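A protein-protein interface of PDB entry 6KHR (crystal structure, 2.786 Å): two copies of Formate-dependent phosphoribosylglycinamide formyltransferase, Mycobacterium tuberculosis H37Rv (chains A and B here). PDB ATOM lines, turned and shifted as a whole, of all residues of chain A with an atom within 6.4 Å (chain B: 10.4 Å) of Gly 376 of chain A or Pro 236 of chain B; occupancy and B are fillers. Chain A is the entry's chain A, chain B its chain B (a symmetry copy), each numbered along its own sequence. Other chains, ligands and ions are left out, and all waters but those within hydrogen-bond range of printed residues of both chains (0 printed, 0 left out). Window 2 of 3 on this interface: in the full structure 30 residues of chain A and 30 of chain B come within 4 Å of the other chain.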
ATOM      1  N   LEU A 371     -19.326 -12.516  11.665  1.00  0.00           N
ATOM      2  CA  LEU A 371     -20.493 -13.078  10.992  1.00  0.00           C
ATOM      3  C   LEU A 371     -21.688 -12.132  11.039  1.00  0.00           C
ATOM      4  O   LEU A 371     -22.320 -11.863  10.012  1.00  0.00           O
ATOM      5  CB  LEU A 371     -20.853 -14.415  11.627  1.00  0.00           C
ATOM      6  CG  LEU A 371     -20.951 -15.556  10.633  1.00  0.00           C
ATOM      7  CD1 LEU A 371     -21.931 -16.573  11.165  1.00  0.00           C
ATOM      8  CD2 LEU A 371     -21.324 -15.031   9.246  1.00  0.00           C
ATOM      9  N   THR A 372     -22.040 -11.655  12.231  1.00  0.00           N
ATOM     10  CA  THR A 372     -23.122 -10.686  12.367  1.00  0.00           C
ATOM     11  C   THR A 372     -22.984  -9.541  11.372  1.00  0.00           C
ATOM     12  O   THR A 372     -23.966  -9.126  10.747  1.00  0.00           O
ATOM     13  CB  THR A 372     -23.161 -10.141  13.799  1.00  0.00           C
ATOM     14  OG1 THR A 372     -23.978 -10.993  14.604  1.00  0.00           O
ATOM     15  CG2 THR A 372     -23.737  -8.740  13.829  1.00  0.00           C
ATOM     16  N   GLY A 373     -21.768  -9.021  11.211  1.00  0.00           N
ATOM     17  CA  GLY A 373     -21.577  -7.909  10.303  1.00  0.00           C
ATOM     18  C   GLY A 373     -21.730  -8.324   8.861  1.00  0.00           C
ATOM     19  O   GLY A 373     -22.385  -7.637   8.076  1.00  0.00           O
ATOM     20  N   ALA A 374     -21.148  -9.466   8.501  1.00  0.00           N
ATOM     21  CA  ALA A 374     -21.183  -9.910   7.120  1.00  0.00           C
ATOM     22  C   ALA A 374     -22.617 -10.104   6.623  1.00  0.00           C
ATOM     23  O   ALA A 374     -22.947  -9.686   5.508  1.00  0.00           O
ATOM     24  CB  ALA A 374     -20.361 -11.192   6.981  1.00  0.00           C
ATOM     25  N   LEU A 375     -23.466 -10.721   7.430  1.00  0.00           N
ATOM     26  CA  LEU A 375     -24.856 -11.026   7.026  1.00  0.00           C
ATOM     27  C   LEU A 375     -25.759  -9.808   7.134  1.00  0.00           C
ATOM     28  O   LEU A 375     -26.902  -9.926   6.875  1.00  0.00           O
ATOM     29  CB  LEU A 375     -25.385 -12.154   7.898  1.00  0.00           C
ATOM     30  CG  LEU A 375     -25.356 -13.550   7.306  1.00  0.00           C
ATOM     31  CD1 LEU A 375     -24.645 -13.579   5.986  1.00  0.00           C
ATOM     32  CD2 LEU A 375     -24.712 -14.492   8.270  1.00  0.00           C
ATOM     33  N   GLY A 376     -25.222  -8.663   7.473  1.00  0.00           N
ATOM     34  CA  GLY A 376     -26.019  -7.437   7.515  1.00  0.00           C
ATOM     35  C   GLY A 376     -26.166  -6.863   6.134  1.00  0.00           C
ATOM     36  O   GLY A 376     -27.064  -6.090   5.934  1.00  0.00           O
ATOM     37  N   VAL A 377     -25.273  -7.238   5.233  1.00  0.00           N
ATOM     38  CA  VAL A 377     -25.299  -6.854   3.806  1.00  0.00           C
ATOM     39  C   VAL A 377     -26.493  -7.517   3.146  1.00  0.00           C
ATOM     40  O   VAL A 377     -26.620  -8.695   3.242  1.00  0.00           O
ATOM     41  CB  VAL A 377     -24.005  -7.334   3.148  1.00  0.00           C
ATOM     42  CG1 VAL A 377     -24.071  -7.278   1.646  1.00  0.00           C
ATOM     43  CG2 VAL A 377     -22.803  -6.602   3.672  1.00  0.00           C
ATOM     44  N   PRO A 378     -27.372  -6.773   2.465  1.00  0.00           N
ATOM     45  CA  PRO A 378     -28.525  -7.355   1.799  1.00  0.00           C
ATOM     46  C   PRO A 378     -28.275  -8.448   0.751  1.00  0.00           C
ATOM     47  O   PRO A 378     -27.356  -8.379   0.034  1.00  0.00           O
ATOM     48  CB  PRO A 378     -29.215  -6.173   1.136  1.00  0.00           C
ATOM     49  CG  PRO A 378     -28.226  -5.068   1.192  1.00  0.00           C
ATOM     50  CD  PRO A 378     -27.342  -5.335   2.378  1.00  0.00           C
ATOM     51  N   SER A 380     -27.280 -11.484   1.159  1.00  0.00           N
ATOM     52  CA  SER A 380     -25.979 -12.139   1.314  1.00  0.00           C
ATOM     53  C   SER A 380     -26.087 -13.518   1.951  1.00  0.00           C
ATOM     54  O   SER A 380     -27.058 -13.825   2.568  1.00  0.00           O
ATOM     55  CB  SER A 380     -25.052 -11.241   2.049  1.00  0.00           C
ATOM     56  OG  SER A 380     -25.489 -10.979   3.354  1.00  0.00           O
ATOM     57  N   ARG A 412     -16.098  -7.689   5.666  1.00  0.00           N
ATOM     58  CA  ARG A 412     -16.536  -7.795   7.065  1.00  0.00           C
ATOM     59  C   ARG A 412     -16.163  -9.128   7.691  1.00  0.00           C
ATOM     60  O   ARG A 412     -16.272  -9.280   8.910  1.00  0.00           O
ATOM     61  CB  ARG A 412     -18.060  -7.635   7.214  1.00  0.00           C
ATOM     62  CG  ARG A 412     -18.713  -6.640   6.282  1.00  0.00           C
ATOM     63  CD  ARG A 412     -19.097  -5.353   6.931  1.00  0.00           C
ATOM     64  NE  ARG A 412     -20.543  -5.246   7.096  1.00  0.00           N
ATOM     65  CZ  ARG A 412     -21.320  -4.411   6.414  1.00  0.00           C
ATOM     66  NH1 ARG A 412     -22.627  -4.382   6.644  1.00  0.00           N
ATOM     67  NH2 ARG A 412     -20.795  -3.601   5.508  1.00  0.00           N
ATOM     68  N   LEU B  48     -23.197 -22.036   8.220  1.00  0.00           N
ATOM     69  CA  LEU B  48     -22.876 -20.786   8.891  1.00  0.00           C
ATOM     70  C   LEU B  48     -21.765 -20.956   9.907  1.00  0.00           C
ATOM     71  O   LEU B  48     -21.442 -19.994  10.606  1.00  0.00           O
ATOM     72  CB  LEU B  48     -24.116 -20.210   9.579  1.00  0.00           C
ATOM     73  CG  LEU B  48     -25.345 -19.787   8.772  1.00  0.00           C
ATOM     74  CD1 LEU B  48     -26.560 -19.501   9.694  1.00  0.00           C
ATOM     75  CD2 LEU B  48     -25.035 -18.570   7.936  1.00  0.00           C
ATOM     76  N   SER B 233     -35.384 -12.283  14.709  1.00  0.00           N
ATOM     77  CA  SER B 233     -33.959 -12.408  14.941  1.00  0.00           C
ATOM     78  C   SER B 233     -33.413 -11.050  15.346  1.00  0.00           C
ATOM     79  O   SER B 233     -34.157 -10.102  15.618  1.00  0.00           O
ATOM     80  CB  SER B 233     -33.231 -12.956  13.709  1.00  0.00           C
ATOM     81  OG  SER B 233     -31.875 -13.210  14.025  1.00  0.00           O
ATOM     82  N   GLN B 234     -32.097 -10.974  15.413  1.00  0.00           N
ATOM     83  CA  GLN B 234     -31.398  -9.712  15.538  1.00  0.00           C
ATOM     84  C   GLN B 234     -30.760  -9.410  14.185  1.00  0.00           C
ATOM     85  O   GLN B 234     -30.313 -10.323  13.484  1.00  0.00           O
ATOM     86  CB  GLN B 234     -30.356  -9.766  16.662  1.00  0.00           C
ATOM     87  CG  GLN B 234     -30.703  -8.904  17.913  1.00  0.00           C
ATOM     88  CD  GLN B 234     -31.759  -9.527  18.837  1.00  0.00           C
ATOM     89  OE1 GLN B 234     -32.895  -9.044  18.923  1.00  0.00           O
ATOM     90  NE2 GLN B 234     -31.379 -10.582  19.549  1.00  0.00           N
ATOM     91  N   GLY B 235     -30.791  -8.143  13.796  1.00  0.00           N
ATOM     92  CA  GLY B 235     -30.040  -7.706  12.645  1.00  0.00           C
ATOM     93  C   GLY B 235     -28.744  -7.072  13.102  1.00  0.00           C
ATOM     94  O   GLY B 235     -28.403  -7.117  14.287  1.00  0.00           O
ATOM     95  N   PRO B 236     -27.988  -6.466  12.179  1.00  0.00           N
ATOM     96  CA  PRO B 236     -26.849  -5.641  12.602  1.00  0.00           C
ATOM     97  C   PRO B 236     -27.257  -4.382  13.367  1.00  0.00           C
ATOM     98  O   PRO B 236     -26.375  -3.658  13.839  1.00  0.00           O
ATOM     99  CB  PRO B 236     -26.153  -5.301  11.273  1.00  0.00           C
ATOM    100  CG  PRO B 236     -27.227  -5.401  10.253  1.00  0.00           C
ATOM    101  CD  PRO B 236     -28.114  -6.526  10.714  1.00  0.00           C
ATOM    102  N   ASN B 237     -28.573  -4.128  13.523  1.00  0.00           N
ATOM    103  CA  ASN B 237     -29.124  -2.980  14.244  1.00  0.00           C
ATOM    104  C   ASN B 237     -30.153  -3.403  15.290  1.00  0.00           C
ATOM    105  O   ASN B 237     -31.020  -2.610  15.675  1.00  0.00           O
ATOM    106  CB  ASN B 237     -29.747  -1.978  13.270  1.00  0.00           C
ATOM    107  CG  ASN B 237     -30.050  -0.645  13.925  1.00  0.00           C
ATOM    108  OD1 ASN B 237     -31.203  -0.356  14.265  1.00  0.00           O
ATOM    109  ND2 ASN B 237     -29.015   0.167  14.118  1.00  0.00           N
ATOM    110  N   GLY B 238     -30.087  -4.645  15.754  1.00  0.00           N
ATOM    111  CA  GLY B 238     -30.963  -5.105  16.807  1.00  0.00           C
ATOM    112  C   GLY B 238     -32.104  -5.985  16.325  1.00  0.00           C
ATOM    113  O   GLY B 238     -31.989  -6.718  15.332  1.00  0.00           O
ATOM    114  N   PRO B 239     -33.239  -5.900  17.015  1.00  0.00           N
ATOM    115  CA  PRO B 239     -34.327  -6.854  16.761  1.00  0.00           C
ATOM    116  C   PRO B 239     -34.934  -6.674  15.377  1.00  0.00           C
ATOM    117  O   PRO B 239     -35.106  -5.554  14.890  1.00  0.00           O
ATOM    118  CB  PRO B 239     -35.348  -6.536  17.859  1.00  0.00           C
ATOM    119  CG  PRO B 239     -34.608  -5.691  18.849  1.00  0.00           C
ATOM    120  CD  PRO B 239     -33.590  -4.940  18.065  1.00  0.00           C
ATOM    121  N   LEU B 240     -35.238  -7.808  14.746  1.00  0.00           N
ATOM    122  CA  LEU B 240     -35.941  -7.868  13.482  1.00  0.00           C
ATOM    123  C   LEU B 240     -37.197  -8.707  13.662  1.00  0.00           C
ATOM    124  O   LEU B 240     -37.175  -9.724  14.362  1.00  0.00           O
ATOM    125  CB  LEU B 240     -35.072  -8.493  12.393  1.00  0.00           C
ATOM    126  CG  LEU B 240     -33.749  -7.841  12.004  1.00  0.00           C
ATOM    127  CD1 LEU B 240     -33.076  -8.667  10.921  1.00  0.00           C
ATOM    128  CD2 LEU B 240     -33.985  -6.423  11.522  1.00  0.00           C
ATOM    129  N   GLU B 242     -39.791 -10.268  10.753  1.00  0.00           N
ATOM    130  CA  GLU B 242     -40.101 -10.394   9.341  1.00  0.00           C
ATOM    131  C   GLU B 242     -41.274 -11.338   9.140  1.00  0.00           C
ATOM    132  O   GLU B 242     -41.454 -12.294   9.900  1.00  0.00           O
ATOM    133  CB  GLU B 242     -38.913 -10.945   8.557  1.00  0.00           C
ATOM    134  CG  GLU B 242     -37.612 -10.248   8.815  1.00  0.00           C
ATOM    135  CD  GLU B 242     -37.343  -9.185   7.800  1.00  0.00           C
ATOM    136  OE1 GLU B 242     -38.154  -8.239   7.713  1.00  0.00           O
ATOM    137  OE2 GLU B 242     -36.335  -9.301   7.074  1.00  0.00           O
ATOM    138  N   ARG B 322     -35.730 -17.107  -1.280  1.00  0.00           N
ATOM    139  CA  ARG B 322     -34.277 -16.981  -1.187  1.00  0.00           C
ATOM    140  C   ARG B 322     -33.725 -17.786  -0.008  1.00  0.00           C
ATOM    141  O   ARG B 322     -32.800 -18.587  -0.167  1.00  0.00           O
ATOM    142  CB  ARG B 322     -33.885 -15.508  -1.069  1.00  0.00           C
ATOM    143  CG  ARG B 322     -32.436 -15.215  -1.385  1.00  0.00           C
ATOM    144  CD  ARG B 322     -32.076 -13.745  -1.126  1.00  0.00           C
ATOM    145  NE  ARG B 322     -31.870 -13.491   0.303  1.00  0.00           N
ATOM    146  CZ  ARG B 322     -30.700 -13.559   0.952  1.00  0.00           C
ATOM    147  NH1 ARG B 322     -29.582 -13.876   0.337  1.00  0.00           N
ATOM    148  NH2 ARG B 322     -30.660 -13.295   2.242  1.00  0.00           N
ATOM    149  N   LEU B 323     -34.284 -17.597   1.181  1.00  0.00           N
ATOM    150  CA  LEU B 323     -33.876 -18.325   2.382  1.00  0.00           C
ATOM    151  C   LEU B 323     -35.013 -19.240   2.822  1.00  0.00           C
ATOM    152  O   LEU B 323     -36.132 -18.777   3.086  1.00  0.00           O
ATOM    153  CB  LEU B 323     -33.507 -17.358   3.508  1.00  0.00           C
ATOM    154  CG  LEU B 323     -32.433 -16.318   3.138  1.00  0.00           C
ATOM    155  CD1 LEU B 323     -32.058 -15.424   4.311  1.00  0.00           C
ATOM    156  CD2 LEU B 323     -31.201 -17.020   2.635  1.00  0.00           C
ATOM    157  N   ARG B 331     -30.459 -18.850  10.931  1.00  0.00           N
ATOM    158  CA  ARG B 331     -30.026 -17.478  11.207  1.00  0.00           C
ATOM    159  C   ARG B 331     -30.661 -16.921  12.482  1.00  0.00           C
ATOM    160  O   ARG B 331     -29.988 -16.217  13.253  1.00  0.00           O
ATOM    161  CB  ARG B 331     -30.320 -16.570  10.018  1.00  0.00           C
ATOM    162  CG  ARG B 331     -29.552 -16.962   8.785  1.00  0.00           C
ATOM    163  CD  ARG B 331     -29.645 -15.888   7.699  1.00  0.00           C
ATOM    164  NE  ARG B 331     -28.968 -16.287   6.467  1.00  0.00           N
ATOM    165  CZ  ARG B 331     -28.585 -15.445   5.508  1.00  0.00           C
ATOM    166  NH1 ARG B 331     -28.810 -14.143   5.630  1.00  0.00           N
ATOM    167  NH2 ARG B 331     -27.976 -15.911   4.428  1.00  0.00           N
ATOM    168  N   LEU B 334     -28.993 -18.168  15.730  1.00  0.00           N
ATOM    169  CA  LEU B 334     -27.690 -17.564  15.919  1.00  0.00           C
ATOM    170  C   LEU B 334     -27.749 -16.042  15.974  1.00  0.00           C
ATOM    171  O   LEU B 334     -26.703 -15.406  16.147  1.00  0.00           O
ATOM    172  CB  LEU B 334     -26.738 -18.013  14.795  1.00  0.00           C
ATOM    173  CG  LEU B 334     -26.365 -19.500  14.654  1.00  0.00           C
ATOM    174  CD1 LEU B 334     -25.482 -19.692  13.445  1.00  0.00           C
ATOM    175  CD2 LEU B 334     -25.676 -20.069  15.902  1.00  0.00           C
ATOM    176  N   GLY B 335     -28.927 -15.443  15.803  1.00  0.00           N
ATOM    177  CA  GLY B 335     -29.060 -14.000  15.964  1.00  0.00           C
ATOM    178  C   GLY B 335     -28.506 -13.195  14.809  1.00  0.00           C
ATOM    179  O   GLY B 335     -27.931 -12.119  15.018  1.00  0.00           O
ATOM    180  N   LEU B 336     -28.664 -13.690  13.596  1.00  0.00           N
ATOM    181  CA  LEU B 336     -28.170 -13.024  12.409  1.00  0.00           C
ATOM    182  C   LEU B 336     -29.327 -12.416  11.611  1.00  0.00           C
ATOM    183  O   LEU B 336     -30.494 -12.780  11.787  1.00  0.00           O
ATOM    184  CB  LEU B 336     -27.371 -14.016  11.550  1.00  0.00           C
ATOM    185  CG  LEU B 336     -26.249 -14.735  12.312  1.00  0.00           C
ATOM    186  CD1 LEU B 336     -25.712 -15.931  11.520  1.00  0.00           C
ATOM    187  CD2 LEU B 336     -25.124 -13.762  12.654  1.00  0.00           C
ATOM    188  N   ALA B 337     -28.982 -11.498  10.710  1.00  0.00           N
ATOM    189  CA  ALA B 337     -29.963 -10.821   9.877  1.00  0.00           C
ATOM    190  C   ALA B 337     -30.661 -11.783   8.926  1.00  0.00           C
ATOM    191  O   ALA B 337     -30.097 -12.796   8.494  1.00  0.00           O
ATOM    192  CB  ALA B 337     -29.294  -9.711   9.073  1.00  0.00           C
ATOM    193  N   VAL B 338     -31.912 -11.457   8.601  1.00  0.00           N
ATOM    194  CA  VAL B 338     -32.702 -12.247   7.670  1.00  0.00           C
ATOM    195  C   VAL B 338     -33.491 -11.320   6.759  1.00  0.00           C
ATOM    196  O   VAL B 338     -33.667 -10.132   7.036  1.00  0.00           O
ATOM    197  CB  VAL B 338     -33.676 -13.220   8.380  1.00  0.00           C
ATOM    198  CG1 VAL B 338     -32.923 -14.316   9.109  1.00  0.00           C
ATOM    199  CG2 VAL B 338     -34.593 -12.473   9.322  1.00  0.00           C
ATOM    200  N   ASP B 339     -33.954 -11.886   5.651  1.00  0.00           N
ATOM    201  CA  ASP B 339     -34.959 -11.277   4.797  1.00  0.00           C
ATOM    202  C   ASP B 339     -35.935 -12.378   4.421  1.00  0.00           C
ATOM    203  O   ASP B 339     -35.679 -13.557   4.672  1.00  0.00           O
ATOM    204  CB  ASP B 339     -34.344 -10.617   3.545  1.00  0.00           C
ATOM    205  CG  ASP B 339     -33.689 -11.631   2.576  1.00  0.00           C
ATOM    206  OD1 ASP B 339     -34.388 -12.525   2.051  1.00  0.00           O
ATOM    207  OD2 ASP B 339     -32.468 -11.511   2.318  1.00  0.00           O
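The guanidinium group (NH1) of Arg 322 of chain B sits at hydrogen-bond distance from the backbone carbonyl oxygen (O) of Ser 380 of chain A (3.4 Å). NH2 of Arg 331 of chain B is in hydrogen-bond range of O of Ser 380 of chain A (2.9 Å).
The side-chain hydroxyl (OG) of Ser 380 of chain A lies within hydrogen-bond range of the backbone carbonyl oxygen (O) of Val 377 of chain A, at 2.6 Å. The backbone carbonyl oxygen (O) of Leu 336 of chain B sits at hydrogen-bond distance from the side-chain hydroxyl (OG) of Ser 233 of chain B, 2.7 Å away. The backbone NH (N) of Ala 337 of chain B is in hydrogen-bond range of the backbone carbonyl oxygen (O) of Gln 234 of chain B. The guanidinium group (NH2) of Arg 322 of chain B lies within salt-bridge range of the side-chain carboxylate (OD2) of Asp 339 of chain B, 2.5 Å away. The backbone NH (N) of Leu 336 of chain B is in hydrogen-bond range of the backbone carbonyl oxygen (O) of Arg 331 of chain B (2.9 Å). The backbone carbonyl oxygen of Ala 337 of chain B lies close to the guanidinium group of Arg 331 of chain B.
Among the printed residues, merely in contact across the chains: Leu 371 of chain A with Leu 48 of chain B (3.5 Å), Leu 371 of chain A with Leu 336 of chain B (3.9 Å), Thr 372 of chain A with Leu 336 of chain B (3.6 Å), Leu 375 of chain A with Arg 331 of chain B (3.9 Å), Leu 375 of chain A with Leu 336 of chain B (3.7 Å), Leu 375 of chain A with Ala 337 of chain B (3.3 Å) and Gly 376 of chain A with Pro 236 of chain B (3.6 Å).
Of the printed residues of chain B, Thr 372 of chain A touches Leu 336. No residue of chain B comes within 4 Å of Gly 373 of chain A. No residue of chain B comes within 4 Å of Ala 374 of chain A. Leu 375 of chain A touches three residues of chain B. Gly 376 of chain A touches just one residue of chain B: Pro 236 (3.6 Å). No residue of chain B comes within 4 Å of Val 377 of chain A. No residue of chain B comes within 4 Å of Pro 378 of chain A. Printed residues of chain B within 4 Å of Ser 380 of chain A: Arg 322 (3.4 Å) and Arg 331 (2.9 Å). Printed residues of chain A within 4 Å of Leu 48 of chain B: Leu 371. Pro 236 of chain B touches just one residue of chain A: Gly 376. Asn 237 of chain B touches none of the printed residues of chain A. Pro 239 of chain B touches none of the printed residues of chain A. Of the printed residues of chain A, Leu 336 of chain B touches Leu 371, Thr 372 and Leu 375. Of the printed residues of chain A, Ala 337 of chain B touches Leu 375. The nearest residue of chain B that does not touch Gly 376 of chain A is Ala 337 of chain B (4.3 Å). The nearest printed residue of chain A that does not touch Leu 48 of chain B is Leu 375 of chain A (4.1 Å).
Hydrophobic or aromatic side chains of chain B within 4 Å of the printed part of chain A: Pro 236, Leu 336 and Ala 337. Of the 10 printed residues of chain A, 5 touch a printed residue of chain B. Among the printed residues, 9 pairs touch across the chains. Among the printed residues, no Asp or Glu carboxylate lies within 4 Å of a Lys or Arg side-chain nitrogen of the other chain.
No position is printed for both chains. Of the 9 pairs that touch across the chains among the printed residues, none has its exchanged pair printed and touching as well.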
